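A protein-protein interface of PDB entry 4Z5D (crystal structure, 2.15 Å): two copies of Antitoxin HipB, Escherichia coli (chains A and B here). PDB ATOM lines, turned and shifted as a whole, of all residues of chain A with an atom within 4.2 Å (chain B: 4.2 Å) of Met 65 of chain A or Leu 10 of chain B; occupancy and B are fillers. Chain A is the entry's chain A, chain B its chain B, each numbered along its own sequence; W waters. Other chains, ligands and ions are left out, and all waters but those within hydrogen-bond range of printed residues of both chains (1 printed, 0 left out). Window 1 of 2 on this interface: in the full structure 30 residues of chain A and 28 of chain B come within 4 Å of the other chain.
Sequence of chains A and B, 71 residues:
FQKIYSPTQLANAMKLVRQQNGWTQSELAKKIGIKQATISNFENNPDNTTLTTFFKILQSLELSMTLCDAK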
ATOM      1  N   PHE A  54       0.466 -13.507 -26.862  1.00  0.00           N
ATOM      2  CA  PHE A  54       0.028 -12.745 -25.717  1.00  0.00           C
ATOM      3  C   PHE A  54      -1.508 -12.644 -25.728  1.00  0.00           C
ATOM      4  O   PHE A  54      -2.147 -12.939 -24.750  1.00  0.00           O
ATOM      5  CB  PHE A  54       0.682 -11.366 -25.756  1.00  0.00           C
ATOM      6  CG  PHE A  54      -0.067 -10.285 -25.030  1.00  0.00           C
ATOM      7  CD1 PHE A  54      -0.407 -10.419 -23.708  1.00  0.00           C
ATOM      8  CD2 PHE A  54      -0.402  -9.127 -25.677  1.00  0.00           C
ATOM      9  CE1 PHE A  54      -1.075  -9.420 -23.044  1.00  0.00           C
ATOM     10  CE2 PHE A  54      -1.073  -8.117 -25.024  1.00  0.00           C
ATOM     11  CZ  PHE A  54      -1.421  -8.268 -23.710  1.00  0.00           C
ATOM     12  N   PHE A  55      -2.072 -12.300 -26.871  1.00  0.00           N
ATOM     13  CA  PHE A  55      -3.509 -12.229 -27.026  1.00  0.00           C
ATOM     14  C   PHE A  55      -4.229 -13.571 -26.827  1.00  0.00           C
ATOM     15  O   PHE A  55      -5.275 -13.612 -26.220  1.00  0.00           O
ATOM     16  CB  PHE A  55      -3.923 -11.535 -28.325  1.00  0.00           C
ATOM     17  CG  PHE A  55      -3.918 -10.039 -28.232  1.00  0.00           C
ATOM     18  CD1 PHE A  55      -4.959  -9.367 -27.639  1.00  0.00           C
ATOM     19  CD2 PHE A  55      -2.863  -9.315 -28.721  1.00  0.00           C
ATOM     20  CE1 PHE A  55      -4.953  -8.003 -27.538  1.00  0.00           C
ATOM     21  CE2 PHE A  55      -2.849  -7.945 -28.635  1.00  0.00           C
ATOM     22  CZ  PHE A  55      -3.882  -7.288 -28.030  1.00  0.00           C
ATOM     23  N   LEU A  58      -4.283 -14.108 -23.073  1.00  0.00           N
ATOM     24  CA  LEU A  58      -5.257 -13.231 -22.459  1.00  0.00           C
ATOM     25  C   LEU A  58      -6.671 -13.804 -22.609  1.00  0.00           C
ATOM     26  O   LEU A  58      -7.413 -13.850 -21.674  1.00  0.00           O
ATOM     27  CB  LEU A  58      -5.230 -11.877 -23.146  1.00  0.00           C
ATOM     28  CG  LEU A  58      -4.271 -10.765 -22.768  1.00  0.00           C
ATOM     29  CD1 LEU A  58      -4.529  -9.596 -23.700  1.00  0.00           C
ATOM     30  CD2 LEU A  58      -4.402 -10.353 -21.316  1.00  0.00           C
ATOM     31  N   SER A  64      -8.836  -9.077 -21.160  1.00  0.00           N
ATOM     32  CA  SER A  64      -8.598  -8.196 -22.263  1.00  0.00           C
ATOM     33  C   SER A  64      -7.644  -7.135 -21.761  1.00  0.00           C
ATOM     34  O   SER A  64      -7.214  -7.189 -20.643  1.00  0.00           O
ATOM     35  CB  SER A  64      -9.881  -7.574 -22.772  1.00  0.00           C
ATOM     36  OG  SER A  64      -9.630  -6.818 -23.914  1.00  0.00           O
ATOM     37  N   MET A  65      -7.260  -6.235 -22.638  1.00  0.00           N
ATOM     38  CA  MET A  65      -6.436  -5.100 -22.285  1.00  0.00           C
ATOM     39  C   MET A  65      -6.950  -3.786 -22.852  1.00  0.00           C
ATOM     40  O   MET A  65      -7.736  -3.752 -23.777  1.00  0.00           O
ATOM     41  CB  MET A  65      -4.993  -5.306 -22.719  1.00  0.00           C
ATOM     42  CG  MET A  65      -4.833  -5.716 -24.155  1.00  0.00           C
ATOM     43  SD  MET A  65      -3.542  -4.818 -24.991  1.00  0.00           S
ATOM     44  CE  MET A  65      -4.057  -3.147 -24.753  1.00  0.00           C
ATOM     45  N   THR A  66      -6.484  -2.712 -22.253  1.00  0.00           N
ATOM     46  CA  THR A  66      -6.769  -1.389 -22.666  1.00  0.00           C
ATOM     47  C   THR A  66      -5.526  -0.532 -22.622  1.00  0.00           C
ATOM     48  O   THR A  66      -4.726  -0.669 -21.775  1.00  0.00           O
ATOM     49  CB  THR A  66      -7.849  -0.777 -21.767  1.00  0.00           C
ATOM     50  OG1 THR A  66      -8.237   0.458 -22.294  1.00  0.00           O
ATOM     51  CG2 THR A  66      -7.360  -0.570 -20.386  1.00  0.00           C
ATOM     52  N   LEU A  67      -5.414   0.380 -23.553  1.00  0.00           N
ATOM     53  CA  LEU A  67      -4.389   1.369 -23.533  1.00  0.00           C
ATOM     54  C   LEU A  67      -4.758   2.458 -22.523  1.00  0.00           C
ATOM     55  O   LEU A  67      -5.899   2.554 -22.205  1.00  0.00           O
ATOM     56  CB  LEU A  67      -4.244   1.946 -24.896  1.00  0.00           C
ATOM     57  CG  LEU A  67      -3.817   1.060 -26.039  1.00  0.00           C
ATOM     58  CD1 LEU A  67      -3.973   1.867 -27.288  1.00  0.00           C
ATOM     59  CD2 LEU A  67      -2.411   0.556 -25.879  1.00  0.00           C
ATOM     60  N   GLN B   2     -10.646   1.906 -25.029  1.00  0.00           N
ATOM     61  CA  GLN B   2     -11.533   0.750 -24.975  1.00  0.00           C
ATOM     62  C   GLN B   2     -10.768  -0.570 -24.900  1.00  0.00           C
ATOM     63  O   GLN B   2      -9.534  -0.590 -24.975  1.00  0.00           O
ATOM     64  CB  GLN B   2     -12.432   0.731 -26.204  1.00  0.00           C
ATOM     65  CG  GLN B   2     -11.673   0.620 -27.510  1.00  0.00           C
ATOM     66  CD  GLN B   2     -12.600   0.519 -28.702  1.00  0.00           C
ATOM     67  OE1 GLN B   2     -12.985   1.528 -29.291  1.00  0.00           O
ATOM     68  NE2 GLN B   2     -12.971  -0.704 -29.058  1.00  0.00           N
ATOM     69  N   LYS B   3     -11.506  -1.672 -24.766  1.00  0.00           N
ATOM     70  CA  LYS B   3     -10.894  -2.996 -24.698  1.00  0.00           C
ATOM     71  C   LYS B   3     -10.348  -3.406 -26.057  1.00  0.00           C
ATOM     72  O   LYS B   3     -10.959  -3.131 -27.087  1.00  0.00           O
ATOM     73  CB  LYS B   3     -11.895  -4.037 -24.191  1.00  0.00           C
ATOM     74  CG  LYS B   3     -12.362  -3.804 -22.757  1.00  0.00           C
ATOM     75  CD  LYS B   3     -13.298  -4.911 -22.304  1.00  0.00           C
ATOM     76  CE  LYS B   3     -13.873  -4.630 -20.922  1.00  0.00           C
ATOM     77  NZ  LYS B   3     -14.751  -5.753 -20.446  1.00  0.00           N
ATOM     78  N   ILE B   4      -9.185  -4.048 -26.049  1.00  0.00           N
ATOM     79  CA  ILE B   4      -8.496  -4.440 -27.274  1.00  0.00           C
ATOM     80  C   ILE B   4      -8.389  -5.958 -27.305  1.00  0.00           C
ATOM     81  O   ILE B   4      -7.985  -6.570 -26.310  1.00  0.00           O
ATOM     82  CB  ILE B   4      -7.070  -3.858 -27.313  1.00  0.00           C
ATOM     83  CG1 ILE B   4      -7.102  -2.335 -27.150  1.00  0.00           C
ATOM     84  CG2 ILE B   4      -6.367  -4.241 -28.608  1.00  0.00           C
ATOM     85  CD1 ILE B   4      -7.660  -1.625 -28.342  1.00  0.00           C
ATOM     86  N   SER B   6      -7.143  -7.978 -30.254  1.00  0.00           N
ATOM     87  CA  SER B   6      -6.199  -8.619 -31.168  1.00  0.00           C
ATOM     88  C   SER B   6      -5.019  -7.705 -31.482  1.00  0.00           C
ATOM     89  O   SER B   6      -5.096  -6.500 -31.254  1.00  0.00           O
ATOM     90  CB  SER B   6      -6.908  -9.002 -32.469  1.00  0.00           C
ATOM     91  OG  SER B   6      -7.201  -7.844 -33.221  1.00  0.00           O
ATOM     92  N   PRO B   7      -3.920  -8.282 -32.000  1.00  0.00           N
ATOM     93  CA  PRO B   7      -2.775  -7.475 -32.420  1.00  0.00           C
ATOM     94  C   PRO B   7      -3.166  -6.444 -33.473  1.00  0.00           C
ATOM     95  O   PRO B   7      -2.695  -5.312 -33.401  1.00  0.00           O
ATOM     96  CB  PRO B   7      -1.828  -8.517 -33.027  1.00  0.00           C
ATOM     97  CG  PRO B   7      -2.131  -9.772 -32.269  1.00  0.00           C
ATOM     98  CD  PRO B   7      -3.634  -9.729 -32.102  1.00  0.00           C
ATOM     99  N   THR B   8      -4.022  -6.820 -34.422  1.00  0.00           N
ATOM    100  CA  THR B   8      -4.439  -5.887 -35.463  1.00  0.00           C
ATOM    101  C   THR B   8      -5.153  -4.682 -34.862  1.00  0.00           C
ATOM    102  O   THR B   8      -4.855  -3.541 -35.194  1.00  0.00           O
ATOM    103  CB  THR B   8      -5.389  -6.551 -36.478  1.00  0.00           C
ATOM    104  OG1 THR B   8      -4.718  -7.646 -37.103  1.00  0.00           O
ATOM    105  CG2 THR B   8      -5.792  -5.555 -37.553  1.00  0.00           C
ATOM    106  N   GLN B   9      -6.119  -4.949 -33.993  1.00  0.00           N
ATOM    107  CA  GLN B   9      -6.835  -3.885 -33.308  1.00  0.00           C
ATOM    108  C   GLN B   9      -5.863  -3.020 -32.514  1.00  0.00           C
ATOM    109  O   GLN B   9      -5.945  -1.794 -32.547  1.00  0.00           O
ATOM    110  CB  GLN B   9      -7.895  -4.481 -32.378  1.00  0.00           C
ATOM    111  CG  GLN B   9      -8.982  -3.497 -31.958  1.00  0.00           C
ATOM    112  CD  GLN B   9     -10.043  -4.143 -31.085  1.00  0.00           C
ATOM    113  OE1 GLN B   9      -9.959  -5.330 -30.744  1.00  0.00           O
ATOM    114  NE2 GLN B   9     -11.053  -3.362 -30.717  1.00  0.00           N
ATOM    115  N   LEU B  10      -4.922  -3.667 -31.827  1.00  0.00           N
ATOM    116  CA  LEU B  10      -3.932  -2.961 -31.015  1.00  0.00           C
ATOM    117  C   LEU B  10      -3.075  -2.033 -31.860  1.00  0.00           C
ATOM    118  O   LEU B  10      -2.883  -0.873 -31.519  1.00  0.00           O
ATOM    119  CB  LEU B  10      -3.019  -3.950 -30.294  1.00  0.00           C
ATOM    120  CG  LEU B  10      -1.910  -3.335 -29.435  1.00  0.00           C
ATOM    121  CD1 LEU B  10      -2.509  -2.526 -28.271  1.00  0.00           C
ATOM    122  CD2 LEU B  10      -0.982  -4.432 -28.911  1.00  0.00           C
ATOM    123  N   ALA B  11      -2.550  -2.557 -32.959  1.00  0.00           N
ATOM    124  CA  ALA B  11      -1.676  -1.780 -33.826  1.00  0.00           C
ATOM    125  C   ALA B  11      -2.436  -0.616 -34.458  1.00  0.00           C
ATOM    126  O   ALA B  11      -1.909   0.483 -34.559  1.00  0.00           O
ATOM    127  CB  ALA B  11      -1.066  -2.673 -34.903  1.00  0.00           C
ATOM    128  N   ASN B  12      -3.673  -0.858 -34.881  1.00  0.00           N
ATOM    129  CA  ASN B  12      -4.490   0.220 -35.449  1.00  0.00           C
ATOM    130  C   ASN B  12      -4.741   1.344 -34.443  1.00  0.00           C
ATOM    131  O   ASN B  12      -4.658   2.524 -34.784  1.00  0.00           O
ATOM    132  CB  ASN B  12      -5.832  -0.301 -35.980  1.00  0.00           C
ATOM    133  CG  ASN B  12      -5.683  -1.182 -37.215  1.00  0.00           C
ATOM    134  OD1 ASN B  12      -4.617  -1.246 -37.830  1.00  0.00           O
ATOM    135  ND2 ASN B  12      -6.768  -1.857 -37.591  1.00  0.00           N
ATOM    136  N   ALA B  13      -5.047   0.985 -33.200  1.00  0.00           N
ATOM    137  CA  ALA B  13      -5.291   2.013 -32.192  1.00  0.00           C
ATOM    138  C   ALA B  13      -4.036   2.837 -31.924  1.00  0.00           C
ATOM    139  O   ALA B  13      -4.102   4.059 -31.860  1.00  0.00           O
ATOM    140  CB  ALA B  13      -5.817   1.405 -30.912  1.00  0.00           C
ATOM    141  N   MET B  14      -2.888   2.177 -31.781  1.00  0.00           N
ATOM    142  CA  MET B  14      -1.645   2.903 -31.521  1.00  0.00           C
ATOM    143  C   MET B  14      -1.209   3.737 -32.725  1.00  0.00           C
ATOM    144  O   MET B  14      -0.588   4.792 -32.565  1.00  0.00           O
ATOM    145  CB  MET B  14      -0.524   1.947 -31.075  1.00  0.00           C
ATOM    146  CG  MET B  14      -0.825   1.279 -29.734  1.00  0.00           C
ATOM    147  SD  MET B  14       0.243  -0.102 -29.306  1.00  0.00           S
ATOM    148  CE  MET B  14       1.844   0.684 -29.197  1.00  0.00           C
ATOM    149  N   PHE B  54       6.531  -3.891 -28.686  1.00  0.00           N
ATOM    150  CA  PHE B  54       5.258  -3.290 -28.345  1.00  0.00           C
ATOM    151  C   PHE B  54       5.422  -2.313 -27.177  1.00  0.00           C
ATOM    152  O   PHE B  54       4.919  -1.213 -27.229  1.00  0.00           O
ATOM    153  CB  PHE B  54       4.252  -4.394 -28.003  1.00  0.00           C
ATOM    154  CG  PHE B  54       3.088  -3.950 -27.180  1.00  0.00           C
ATOM    155  CD1 PHE B  54       2.252  -2.953 -27.616  1.00  0.00           C
ATOM    156  CD2 PHE B  54       2.838  -4.537 -25.969  1.00  0.00           C
ATOM    157  CE1 PHE B  54       1.191  -2.550 -26.857  1.00  0.00           C
ATOM    158  CE2 PHE B  54       1.770  -4.147 -25.201  1.00  0.00           C
ATOM    159  CZ  PHE B  54       0.944  -3.149 -25.647  1.00  0.00           C
ATOM    160  N   THR B  66      -3.184  -1.527 -19.233  1.00  0.00           N
ATOM    161  CA  THR B  66      -3.629  -2.291 -18.095  1.00  0.00           C
ATOM    162  C   THR B  66      -4.445  -3.464 -18.599  1.00  0.00           C
ATOM    163  O   THR B  66      -5.008  -3.423 -19.673  1.00  0.00           O
ATOM    164  CB  THR B  66      -4.498  -1.468 -17.129  1.00  0.00           C
ATOM    165  OG1 THR B  66      -5.707  -1.097 -17.777  1.00  0.00           O
ATOM    166  CG2 THR B  66      -3.793  -0.230 -16.693  1.00  0.00           C
ATOM    167  N   CYS B  68      -7.764  -5.995 -18.026  1.00  0.00           N
ATOM    168  CA  CYS B  68      -9.166  -5.882 -17.645  1.00  0.00           C
ATOM    169  C   CYS B  68      -9.914  -7.174 -17.931  1.00  0.00           C
ATOM    170  O   CYS B  68      -9.402  -8.063 -18.573  1.00  0.00           O
ATOM    171  CB  CYS B  68      -9.852  -4.730 -18.369  1.00  0.00           C
ATOM    172  SG  CYS B  68      -9.872  -4.874 -20.157  1.00  0.00           S
HETATM  173  O   HOH W   1      -7.608   0.959 -25.436  1.00  0.00           O
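The side-chain hydroxyl of Thr 66 of chain A lies within hydrogen-bond range of the backbone carbonyl oxygen of Gln 2 of chain B (3.2 Å).
The backbone NH (N) of Thr 66 of chain A lies within hydrogen-bond range of the backbone carbonyl oxygen (O) of Thr 66 of chain B, 3.1 Å away.
N of Ile 4 of chain B lies within hydrogen-bond range of O of Met 65 of chain A (2.7 Å).
The side-chain hydroxyl of Ser 64 of chain A is in hydrogen-bond range of the backbone carbonyl oxygen of Ile 4 of chain B (2.9 Å).
The backbone carbonyl oxygen of Cys 68 of chain B is in hydrogen-bond range of the backbone NH of Ser 64 of chain A.
The backbone NH (N) of Gln 9 of chain B sits at hydrogen-bond distance from the side-chain hydroxyl (OG) of Ser 6 of chain B, at 3.2 Å.
Phe 55 of chain A touches Ile 4 of chain B (CE1 to O, 3.6 Å).
Ser 6 of chain B touches Phe 55 of chain A.
Pro 7 of chain B touches Phe 55 of chain A.
Leu 10 of chain B touches Phe 55 of chain A (CD2 to CE2, 3.99 Å).
OG of Ser 64 of chain A touches CB of Lys 3 of chain B, 3.6 Å away.
O of Gln 2 of chain B touches O of Met 65 of chain A, 3.8 Å away.
CA of Lys 3 of chain B touches O of Met 65 of chain A (3.4 Å).
Leu 10 of chain B touches Met 65 of chain A (CD1 to CE, 3.9 Å).
CA of Met 65 of chain A touches O of Thr 66 of chain B, at 3.4 Å.
Leu 10 of chain B touches Leu 67 of chain A.
Met 65 of chain A touches just these residues of chain B: Gln 2 (3.8 Å), Lys 3 (3.4 Å), Ile 4 (2.7 Å), Leu 10 (3.9 Å), Thr 66 (3.4 Å) and Cys 68 (3.9 Å).
Printed residues of chain A within 4 Å of Leu 10 of chain B: Phe 55, Met 65 and Leu 67.
Of the printed residues of chain A, Thr 66 of chain B touches Met 65 (3.4 Å) and Thr 66 (3.1 Å).
Of the printed residues of chain A, Ile 4 of chain B touches Phe 55 (3.6 Å), Ser 64 (2.9 Å) and Met 65 (2.7 Å).
Of the printed residues of chain B, Leu 67 of chain A touches Leu 10.
Of the printed residues of chain A, Lys 3 of chain B touches Ser 64 (3.6 Å) and Met 65 (3.4 Å).
Of the printed residues of chain B, Ser 64 of chain A touches Lys 3, Ile 4 and Cys 68.
Gln 9 of chain B touches none of the printed residues of chain A.
The nearest printed residue of chain A that does not touch Leu 10 of chain B is Phe 54 of chain A (5.4 Å).
Hydrophobic or aromatic side chains of chain B that line the printed part of chain A: Ile 4, Pro 7 and Leu 10.
Of the 7 printed residues of chain A, 5 touch a printed residue of chain B.
Hydrophobic or aromatic side chains of chain A that line the printed part of chain B: Phe 55, Met 65 and Leu 67.
Among the printed residues, no Asp or Glu carboxylate lies within 4 Å of a Lys or Arg side-chain nitrogen of the other chain.
Thr 66 of chain B touches its own counterpart, Thr 66 of chain A.
Of the 16 pairs that touch across the chains among the printed residues, 1 has its exchanged pair printed and touching as well.
Water W1 lies within hydrogen-bond range of the backbone carbonyl oxygen (O) of Gln 2 of chain B, the backbone NH (N) of Leu 67 of chain A and the side-chain hydroxyl (OG1) of Thr 66 of chain A.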
